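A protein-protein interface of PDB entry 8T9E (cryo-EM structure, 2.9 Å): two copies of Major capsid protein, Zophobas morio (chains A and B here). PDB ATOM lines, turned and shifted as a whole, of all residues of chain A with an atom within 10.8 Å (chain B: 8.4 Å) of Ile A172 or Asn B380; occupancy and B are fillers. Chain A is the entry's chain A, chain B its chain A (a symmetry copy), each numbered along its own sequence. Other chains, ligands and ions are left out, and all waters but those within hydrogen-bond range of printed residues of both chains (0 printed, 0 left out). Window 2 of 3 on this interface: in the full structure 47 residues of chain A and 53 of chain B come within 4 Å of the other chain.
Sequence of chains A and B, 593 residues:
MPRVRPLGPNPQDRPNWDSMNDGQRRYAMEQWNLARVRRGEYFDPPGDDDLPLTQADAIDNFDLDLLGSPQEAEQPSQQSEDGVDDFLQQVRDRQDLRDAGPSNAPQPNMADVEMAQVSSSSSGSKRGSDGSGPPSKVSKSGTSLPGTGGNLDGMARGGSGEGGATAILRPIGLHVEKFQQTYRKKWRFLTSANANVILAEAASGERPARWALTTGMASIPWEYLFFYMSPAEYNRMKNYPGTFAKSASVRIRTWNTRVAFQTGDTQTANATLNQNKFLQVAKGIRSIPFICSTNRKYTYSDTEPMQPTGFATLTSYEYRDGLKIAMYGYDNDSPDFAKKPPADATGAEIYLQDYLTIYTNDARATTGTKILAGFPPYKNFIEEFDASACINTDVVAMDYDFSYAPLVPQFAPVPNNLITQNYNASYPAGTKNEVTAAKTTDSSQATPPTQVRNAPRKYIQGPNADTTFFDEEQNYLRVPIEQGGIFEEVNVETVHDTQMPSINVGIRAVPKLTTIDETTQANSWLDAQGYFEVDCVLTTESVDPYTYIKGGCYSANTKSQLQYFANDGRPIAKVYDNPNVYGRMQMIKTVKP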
ATOM      1  N   PRO A 171     -14.573  18.435  -5.928  1.00  0.00           N
ATOM      2  CA  PRO A 171     -13.120  18.294  -5.785  1.00  0.00           C
ATOM      3  C   PRO A 171     -12.527  17.366  -6.840  1.00  0.00           C
ATOM      4  O   PRO A 171     -13.271  16.646  -7.501  1.00  0.00           O
ATOM      5  CB  PRO A 171     -12.958  17.703  -4.384  1.00  0.00           C
ATOM      6  CG  PRO A 171     -14.235  17.994  -3.685  1.00  0.00           C
ATOM      7  CD  PRO A 171     -15.293  17.994  -4.724  1.00  0.00           C
ATOM      8  N   ILE A 172     -11.200  17.385  -6.992  1.00  0.00           N
ATOM      9  CA  ILE A 172     -10.562  16.605  -8.044  1.00  0.00           C
ATOM     10  C   ILE A 172     -10.694  15.106  -7.812  1.00  0.00           C
ATOM     11  O   ILE A 172     -10.712  14.335  -8.778  1.00  0.00           O
ATOM     12  CB  ILE A 172      -9.085  17.013  -8.196  1.00  0.00           C
ATOM     13  CG1 ILE A 172      -8.307  16.733  -6.915  1.00  0.00           C
ATOM     14  CG2 ILE A 172      -8.977  18.478  -8.561  1.00  0.00           C
ATOM     15  CD1 ILE A 172      -6.818  16.894  -7.078  1.00  0.00           C
ATOM     16  N   GLY A 173     -10.785  14.667  -6.562  1.00  0.00           N
ATOM     17  CA  GLY A 173     -10.990  13.257  -6.318  1.00  0.00           C
ATOM     18  C   GLY A 173      -9.721  12.431  -6.457  1.00  0.00           C
ATOM     19  O   GLY A 173      -8.601  12.893  -6.235  1.00  0.00           O
ATOM     20  N   LEU A 174      -9.925  11.170  -6.827  1.00  0.00           N
ATOM     21  CA  LEU A 174      -8.826  10.220  -6.923  1.00  0.00           C
ATOM     22  C   LEU A 174      -8.106  10.360  -8.257  1.00  0.00           C
ATOM     23  O   LEU A 174      -8.733  10.599  -9.291  1.00  0.00           O
ATOM     24  CB  LEU A 174      -9.352   8.797  -6.753  1.00  0.00           C
ATOM     25  CG  LEU A 174      -8.314   7.680  -6.727  1.00  0.00           C
ATOM     26  CD1 LEU A 174      -7.430   7.835  -5.512  1.00  0.00           C
ATOM     27  CD2 LEU A 174      -8.985   6.324  -6.736  1.00  0.00           C
ATOM     28  N   HIS A 175      -6.784  10.204  -8.231  1.00  0.00           N
ATOM     29  CA  HIS A 175      -5.985  10.230  -9.449  1.00  0.00           C
ATOM     30  C   HIS A 175      -5.883   8.820 -10.016  1.00  0.00           C
ATOM     31  O   HIS A 175      -5.379   7.912  -9.351  1.00  0.00           O
ATOM     32  CB  HIS A 175      -4.597  10.797  -9.170  1.00  0.00           C
ATOM     33  CG  HIS A 175      -3.737  10.919 -10.389  1.00  0.00           C
ATOM     34  ND1 HIS A 175      -2.364  11.017 -10.325  1.00  0.00           N
ATOM     35  CD2 HIS A 175      -4.056  10.967 -11.704  1.00  0.00           C
ATOM     36  CE1 HIS A 175      -1.875  11.113 -11.549  1.00  0.00           C
ATOM     37  NE2 HIS A 175      -2.881  11.085 -12.403  1.00  0.00           N
ATOM     38  N   VAL A 176      -6.390   8.629 -11.229  1.00  0.00           N
ATOM     39  CA  VAL A 176      -6.303   7.353 -11.927  1.00  0.00           C
ATOM     40  C   VAL A 176      -5.880   7.620 -13.362  1.00  0.00           C
ATOM     41  O   VAL A 176      -6.459   8.475 -14.042  1.00  0.00           O
ATOM     42  CB  VAL A 176      -7.638   6.577 -11.892  1.00  0.00           C
ATOM     43  CG1 VAL A 176      -7.465   5.213 -12.525  1.00  0.00           C
ATOM     44  CG2 VAL A 176      -8.137   6.425 -10.470  1.00  0.00           C
ATOM     45  N   GLU A 177      -4.872   6.889 -13.824  1.00  0.00           N
ATOM     46  CA  GLU A 177      -4.416   6.964 -15.205  1.00  0.00           C
ATOM     47  C   GLU A 177      -4.932   5.754 -15.970  1.00  0.00           C
ATOM     48  O   GLU A 177      -4.696   4.616 -15.563  1.00  0.00           O
ATOM     49  CB  GLU A 177      -2.890   7.018 -15.278  1.00  0.00           C
ATOM     50  CG  GLU A 177      -2.275   8.294 -14.734  1.00  0.00           C
ATOM     51  CD  GLU A 177      -2.657   9.523 -15.537  1.00  0.00           C
ATOM     52  OE1 GLU A 177      -2.995   9.382 -16.730  1.00  0.00           O
ATOM     53  OE2 GLU A 177      -2.619  10.635 -14.971  1.00  0.00           O
ATOM     54  N   LYS A 178      -5.624   6.000 -17.076  1.00  0.00           N
ATOM     55  CA  LYS A 178      -6.193   4.943 -17.900  1.00  0.00           C
ATOM     56  C   LYS A 178      -5.353   4.779 -19.157  1.00  0.00           C
ATOM     57  O   LYS A 178      -5.069   5.762 -19.848  1.00  0.00           O
ATOM     58  CB  LYS A 178      -7.642   5.259 -18.273  1.00  0.00           C
ATOM     59  CG  LYS A 178      -8.675   4.482 -17.482  1.00  0.00           C
ATOM     60  CD  LYS A 178      -9.069   5.225 -16.218  1.00  0.00           C
ATOM     61  CE  LYS A 178     -10.224   4.536 -15.510  1.00  0.00           C
ATOM     62  NZ  LYS A 178     -10.639   5.261 -14.277  1.00  0.00           N
ATOM     63  N   PRO A 545      -3.972   3.584 -10.257  1.00  0.00           N
ATOM     64  CA  PRO A 545      -4.570   4.449  -9.238  1.00  0.00           C
ATOM     65  C   PRO A 545      -3.552   4.904  -8.205  1.00  0.00           C
ATOM     66  O   PRO A 545      -2.695   4.141  -7.756  1.00  0.00           O
ATOM     67  CB  PRO A 545      -5.626   3.534  -8.606  1.00  0.00           C
ATOM     68  CG  PRO A 545      -5.023   2.173  -8.716  1.00  0.00           C
ATOM     69  CD  PRO A 545      -4.103   2.161  -9.910  1.00  0.00           C
ATOM     70  N   TYR A 546      -3.653   6.169  -7.819  1.00  0.00           N
ATOM     71  CA  TYR A 546      -2.791   6.740  -6.796  1.00  0.00           C
ATOM     72  C   TYR A 546      -3.643   7.094  -5.584  1.00  0.00           C
ATOM     73  O   TYR A 546      -4.116   8.218  -5.420  1.00  0.00           O
ATOM     74  CB  TYR A 546      -2.049   7.949  -7.344  1.00  0.00           C
ATOM     75  CG  TYR A 546      -1.204   7.633  -8.550  1.00  0.00           C
ATOM     76  CD1 TYR A 546       0.087   7.151  -8.410  1.00  0.00           C
ATOM     77  CD2 TYR A 546      -1.703   7.805  -9.829  1.00  0.00           C
ATOM     78  CE1 TYR A 546       0.856   6.863  -9.510  1.00  0.00           C
ATOM     79  CE2 TYR A 546      -0.942   7.517 -10.933  1.00  0.00           C
ATOM     80  CZ  TYR A 546       0.338   7.046 -10.770  1.00  0.00           C
ATOM     81  OH  TYR A 546       1.101   6.761 -11.877  1.00  0.00           O
ATOM     82  N   THR A 547      -3.841   6.095  -4.730  1.00  0.00           N
ATOM     83  CA  THR A 547      -4.685   6.240  -3.556  1.00  0.00           C
ATOM     84  C   THR A 547      -3.986   6.946  -2.403  1.00  0.00           C
ATOM     85  O   THR A 547      -4.616   7.762  -1.723  1.00  0.00           O
ATOM     86  CB  THR A 547      -5.177   4.863  -3.117  1.00  0.00           C
ATOM     87  OG1 THR A 547      -6.096   4.353  -4.092  1.00  0.00           O
ATOM     88  CG2 THR A 547      -5.852   4.934  -1.797  1.00  0.00           C
ATOM     89  N   TYR A 548      -2.704   6.677  -2.181  1.00  0.00           N
ATOM     90  CA  TYR A 548      -1.964   7.269  -1.079  1.00  0.00           C
ATOM     91  C   TYR A 548      -0.886   8.189  -1.633  1.00  0.00           C
ATOM     92  O   TYR A 548      -0.564   8.155  -2.822  1.00  0.00           O
ATOM     93  CB  TYR A 548      -1.340   6.195  -0.183  1.00  0.00           C
ATOM     94  CG  TYR A 548      -2.256   5.700   0.914  1.00  0.00           C
ATOM     95  CD1 TYR A 548      -3.489   5.152   0.616  1.00  0.00           C
ATOM     96  CD2 TYR A 548      -1.888   5.787   2.245  1.00  0.00           C
ATOM     97  CE1 TYR A 548      -4.329   4.702   1.608  1.00  0.00           C
ATOM     98  CE2 TYR A 548      -2.722   5.339   3.246  1.00  0.00           C
ATOM     99  CZ  TYR A 548      -3.941   4.797   2.921  1.00  0.00           C
ATOM    100  OH  TYR A 548      -4.779   4.347   3.913  1.00  0.00           O
ATOM    101  N   ILE A 549      -0.331   9.022  -0.753  1.00  0.00           N
ATOM    102  CA  ILE A 549       0.638  10.024  -1.185  1.00  0.00           C
ATOM    103  C   ILE A 549       1.961   9.378  -1.574  1.00  0.00           C
ATOM    104  O   ILE A 549       2.569   9.745  -2.584  1.00  0.00           O
ATOM    105  CB  ILE A 549       0.827  11.090  -0.091  1.00  0.00           C
ATOM    106  CG1 ILE A 549      -0.426  11.954   0.029  1.00  0.00           C
ATOM    107  CG2 ILE A 549       2.031  11.956  -0.389  1.00  0.00           C
ATOM    108  CD1 ILE A 549      -0.357  12.964   1.136  1.00  0.00           C
ATOM    109  N   ILE B 285     -17.423  11.314   3.106  1.00  0.00           N
ATOM    110  CA  ILE B 285     -16.037  10.874   3.220  1.00  0.00           C
ATOM    111  C   ILE B 285     -15.958   9.566   3.995  1.00  0.00           C
ATOM    112  O   ILE B 285     -14.960   8.841   3.914  1.00  0.00           O
ATOM    113  CB  ILE B 285     -15.173  11.976   3.865  1.00  0.00           C
ATOM    114  CG1 ILE B 285     -13.687  11.659   3.708  1.00  0.00           C
ATOM    115  CG2 ILE B 285     -15.523  12.140   5.327  1.00  0.00           C
ATOM    116  CD1 ILE B 285     -12.812  12.879   3.586  1.00  0.00           C
ATOM    117  N   ILE B 288     -15.784   6.399   1.555  1.00  0.00           N
ATOM    118  CA  ILE B 288     -14.657   6.224   0.644  1.00  0.00           C
ATOM    119  C   ILE B 288     -13.831   5.026   1.097  1.00  0.00           C
ATOM    120  O   ILE B 288     -13.362   4.996   2.242  1.00  0.00           O
ATOM    121  CB  ILE B 288     -13.809   7.502   0.564  1.00  0.00           C
ATOM    122  CG1 ILE B 288     -14.654   8.656   0.028  1.00  0.00           C
ATOM    123  CG2 ILE B 288     -12.614   7.287  -0.328  1.00  0.00           C
ATOM    124  CD1 ILE B 288     -13.897   9.945  -0.122  1.00  0.00           C
ATOM    125  N   PHE B 290     -10.796   3.818   0.599  1.00  0.00           N
ATOM    126  CA  PHE B 290      -9.375   3.899   0.901  1.00  0.00           C
ATOM    127  C   PHE B 290      -9.026   4.975   1.918  1.00  0.00           C
ATOM    128  O   PHE B 290      -7.849   5.117   2.261  1.00  0.00           O
ATOM    129  CB  PHE B 290      -8.575   4.136  -0.385  1.00  0.00           C
ATOM    130  CG  PHE B 290      -9.118   5.234  -1.244  1.00  0.00           C
ATOM    131  CD1 PHE B 290      -8.711   6.541  -1.059  1.00  0.00           C
ATOM    132  CD2 PHE B 290     -10.035   4.959  -2.238  1.00  0.00           C
ATOM    133  CE1 PHE B 290      -9.209   7.546  -1.849  1.00  0.00           C
ATOM    134  CE2 PHE B 290     -10.536   5.965  -3.028  1.00  0.00           C
ATOM    135  CZ  PHE B 290     -10.122   7.258  -2.833  1.00  0.00           C
ATOM    136  N   ILE B 291     -10.005   5.732   2.409  1.00  0.00           N
ATOM    137  CA  ILE B 291      -9.766   6.718   3.461  1.00  0.00           C
ATOM    138  C   ILE B 291     -10.318   6.115   4.747  1.00  0.00           C
ATOM    139  O   ILE B 291     -11.527   6.042   4.959  1.00  0.00           O
ATOM    140  CB  ILE B 291     -10.396   8.071   3.138  1.00  0.00           C
ATOM    141  CG1 ILE B 291      -9.836   8.626   1.830  1.00  0.00           C
ATOM    142  CG2 ILE B 291     -10.141   9.051   4.265  1.00  0.00           C
ATOM    143  CD1 ILE B 291     -10.398   9.968   1.454  1.00  0.00           C
ATOM    144  N   PRO B 376      -3.573   9.218   2.869  1.00  0.00           N
ATOM    145  CA  PRO B 376      -4.346   9.526   1.676  1.00  0.00           C
ATOM    146  C   PRO B 376      -4.492  11.033   1.522  1.00  0.00           C
ATOM    147  O   PRO B 376      -4.570  11.765   2.521  1.00  0.00           O
ATOM    148  CB  PRO B 376      -5.700   8.859   1.947  1.00  0.00           C
ATOM    149  CG  PRO B 376      -5.476   7.947   3.096  1.00  0.00           C
ATOM    150  CD  PRO B 376      -4.390   8.562   3.897  1.00  0.00           C
ATOM    151  N   PRO B 377      -4.540  11.522   0.295  1.00  0.00           N
ATOM    152  CA  PRO B 377      -4.747  12.966   0.085  1.00  0.00           C
ATOM    153  C   PRO B 377      -6.209  13.366   0.253  1.00  0.00           C
ATOM    154  O   PRO B 377      -6.918  13.660  -0.710  1.00  0.00           O
ATOM    155  CB  PRO B 377      -4.237  13.160  -1.347  1.00  0.00           C
ATOM    156  CG  PRO B 377      -4.501  11.864  -2.009  1.00  0.00           C
ATOM    157  CD  PRO B 377      -4.313  10.803  -0.968  1.00  0.00           C
ATOM    158  N   TYR B 378      -6.673  13.381   1.506  1.00  0.00           N
ATOM    159  CA  TYR B 378      -8.077  13.662   1.780  1.00  0.00           C
ATOM    160  C   TYR B 378      -8.469  15.085   1.412  1.00  0.00           C
ATOM    161  O   TYR B 378      -9.664  15.392   1.354  1.00  0.00           O
ATOM    162  CB  TYR B 378      -8.394  13.371   3.251  1.00  0.00           C
ATOM    163  CG  TYR B 378      -7.975  14.445   4.231  1.00  0.00           C
ATOM    164  CD1 TYR B 378      -8.811  15.514   4.528  1.00  0.00           C
ATOM    165  CD2 TYR B 378      -6.752  14.376   4.880  1.00  0.00           C
ATOM    166  CE1 TYR B 378      -8.430  16.488   5.420  1.00  0.00           C
ATOM    167  CE2 TYR B 378      -6.367  15.346   5.777  1.00  0.00           C
ATOM    168  CZ  TYR B 378      -7.210  16.398   6.045  1.00  0.00           C
ATOM    169  OH  TYR B 378      -6.827  17.366   6.940  1.00  0.00           O
ATOM    170  N   LYS B 379      -7.496  15.960   1.170  1.00  0.00           N
ATOM    171  CA  LYS B 379      -7.746  17.300   0.660  1.00  0.00           C
ATOM    172  C   LYS B 379      -8.500  17.241  -0.661  1.00  0.00           C
ATOM    173  O   LYS B 379      -9.310  18.122  -0.968  1.00  0.00           O
ATOM    174  CB  LYS B 379      -6.420  18.041   0.488  1.00  0.00           C
ATOM    175  CG  LYS B 379      -6.493  19.334  -0.287  1.00  0.00           C
ATOM    176  CD  LYS B 379      -5.110  19.756  -0.731  1.00  0.00           C
ATOM    177  CE  LYS B 379      -4.550  18.784  -1.744  1.00  0.00           C
ATOM    178  NZ  LYS B 379      -3.223  19.207  -2.263  1.00  0.00           N
ATOM    179  N   ASN B 380      -8.244  16.196  -1.446  1.00  0.00           N
ATOM    180  CA  ASN B 380      -8.826  16.046  -2.771  1.00  0.00           C
ATOM    181  C   ASN B 380     -10.259  15.543  -2.740  1.00  0.00           C
ATOM    182  O   ASN B 380     -10.847  15.338  -3.806  1.00  0.00           O
ATOM    183  CB  ASN B 380      -7.976  15.088  -3.604  1.00  0.00           C
ATOM    184  CG  ASN B 380      -6.563  15.576  -3.788  1.00  0.00           C
ATOM    185  OD1 ASN B 380      -6.246  16.719  -3.473  1.00  0.00           O
ATOM    186  ND2 ASN B 380      -5.700  14.713  -4.300  1.00  0.00           N
ATOM    187  N   PHE B 381     -10.828  15.329  -1.558  1.00  0.00           N
ATOM    188  CA  PHE B 381     -12.160  14.760  -1.426  1.00  0.00           C
ATOM    189  C   PHE B 381     -13.101  15.625  -0.606  1.00  0.00           C
ATOM    190  O   PHE B 381     -14.199  15.170  -0.270  1.00  0.00           O
ATOM    191  CB  PHE B 381     -12.070  13.361  -0.805  1.00  0.00           C
ATOM    192  CG  PHE B 381     -11.234  12.409  -1.602  1.00  0.00           C
ATOM    193  CD1 PHE B 381     -11.798  11.654  -2.611  1.00  0.00           C
ATOM    194  CD2 PHE B 381      -9.879  12.291  -1.362  1.00  0.00           C
ATOM    195  CE1 PHE B 381     -11.030  10.788  -3.349  1.00  0.00           C
ATOM    196  CE2 PHE B 381      -9.108  11.428  -2.101  1.00  0.00           C
ATOM    197  CZ  PHE B 381      -9.685  10.677  -3.095  1.00  0.00           C
ATOM    198  N   ILE B 382     -12.709  16.850  -0.275  1.00  0.00           N
ATOM    199  CA  ILE B 382     -13.533  17.755   0.511  1.00  0.00           C
ATOM    200  C   ILE B 382     -13.667  19.068  -0.245  1.00  0.00           C
ATOM    201  O   ILE B 382     -12.823  19.419  -1.076  1.00  0.00           O
ATOM    202  CB  ILE B 382     -12.951  17.996   1.920  1.00  0.00           C
ATOM    203  CG1 ILE B 382     -11.697  18.861   1.834  1.00  0.00           C
ATOM    204  CG2 ILE B 382     -12.640  16.680   2.605  1.00  0.00           C
ATOM    205  CD1 ILE B 382     -11.163  19.292   3.167  1.00  0.00           C
ATOM    206  N   GLU B 383     -14.744  19.788   0.041  1.00  0.00           N
ATOM    207  CA  GLU B 383     -14.973  21.103  -0.533  1.00  0.00           C
ATOM    208  C   GLU B 383     -14.493  22.181   0.426  1.00  0.00           C
ATOM    209  O   GLU B 383     -14.721  22.099   1.634  1.00  0.00           O
ATOM    210  CB  GLU B 383     -16.454  21.308  -0.843  1.00  0.00           C
ATOM    211  CG  GLU B 383     -16.980  20.410  -1.936  1.00  0.00           C
ATOM    212  CD  GLU B 383     -18.394  20.759  -2.339  1.00  0.00           C
ATOM    213  OE1 GLU B 383     -19.316  20.519  -1.531  1.00  0.00           O
ATOM    214  OE2 GLU B 383     -18.585  21.274  -3.460  1.00  0.00           O
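Among the printed residues, merely in contact across the chains: Pro A171 with Asn B380, Pro A171 with Ile B382, Ile A172 with Asn B380, Gly A173 with Phe B381, Leu A174 with Phe B290, Leu A174 with Phe B381, Thr A547 with Phe B290, Thr A547 with Pro B376, Thr A547 with Pro B377, Tyr A548 with Phe B290 and Tyr A548 with Pro B376.
No position is printed for both chains. Of the 12 pairs that touch across the chains among the printed residues, none has its exchanged pair printed and touching as well.
Of the printed residues of chain B, Pro A171 touches Asn B380 (3.2 Å) and Ile B382 (3.3 Å). Of chain B, only Asn B380 (2.8 Å) and Phe B381 (3.8 Å) come within 4 Å of Gly A173. Printed residues of chain B within 4 Å of Leu A174: Phe B290 and Phe B381. Glu A177 touches none of the printed residues of chain B. Of the printed residues of chain B, Thr A547 touches Phe B290, Pro B376 and Pro B377. Of the printed residues of chain A, Phe B290 touches Leu A174 (3.8 Å), Thr A547 (3.2 Å) and Tyr A548 (3.6 Å). Printed residues of chain A within 4 Å of Pro B376: Thr A547 (3.8 Å) and Tyr A548 (3.5 Å). Of the printed residues of chain A, Pro B377 touches Thr A547 (3.1 Å). No residue of chain A comes within 4 Å of Lys B379. Asn B380 touches just these residues of chain A: Pro A171, Ile A172 and Gly A173. Of the printed residues of chain A, Phe B381 touches Gly A173 (3.8 Å) and Leu A174 (3.7 Å). Printed residues of chain A within 4 Å of Ile B382: Pro A171. The nearest residue of chain A that does not touch Asn B380 is Leu A174 (5.2 Å).
The backbone carbonyl oxygen of Asn B380 sits at hydrogen-bond distance from the backbone NH of Gly A173, 2.8 Å away.
Hydrophobic or aromatic side chains of chain A that line the printed part of chain B: Pro A171, Ile A172, Leu A174 and Tyr A548. Among the printed residues, no Asp or Glu carboxylate lies within 4 Å of a Lys or Arg side-chain nitrogen of the other chain.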
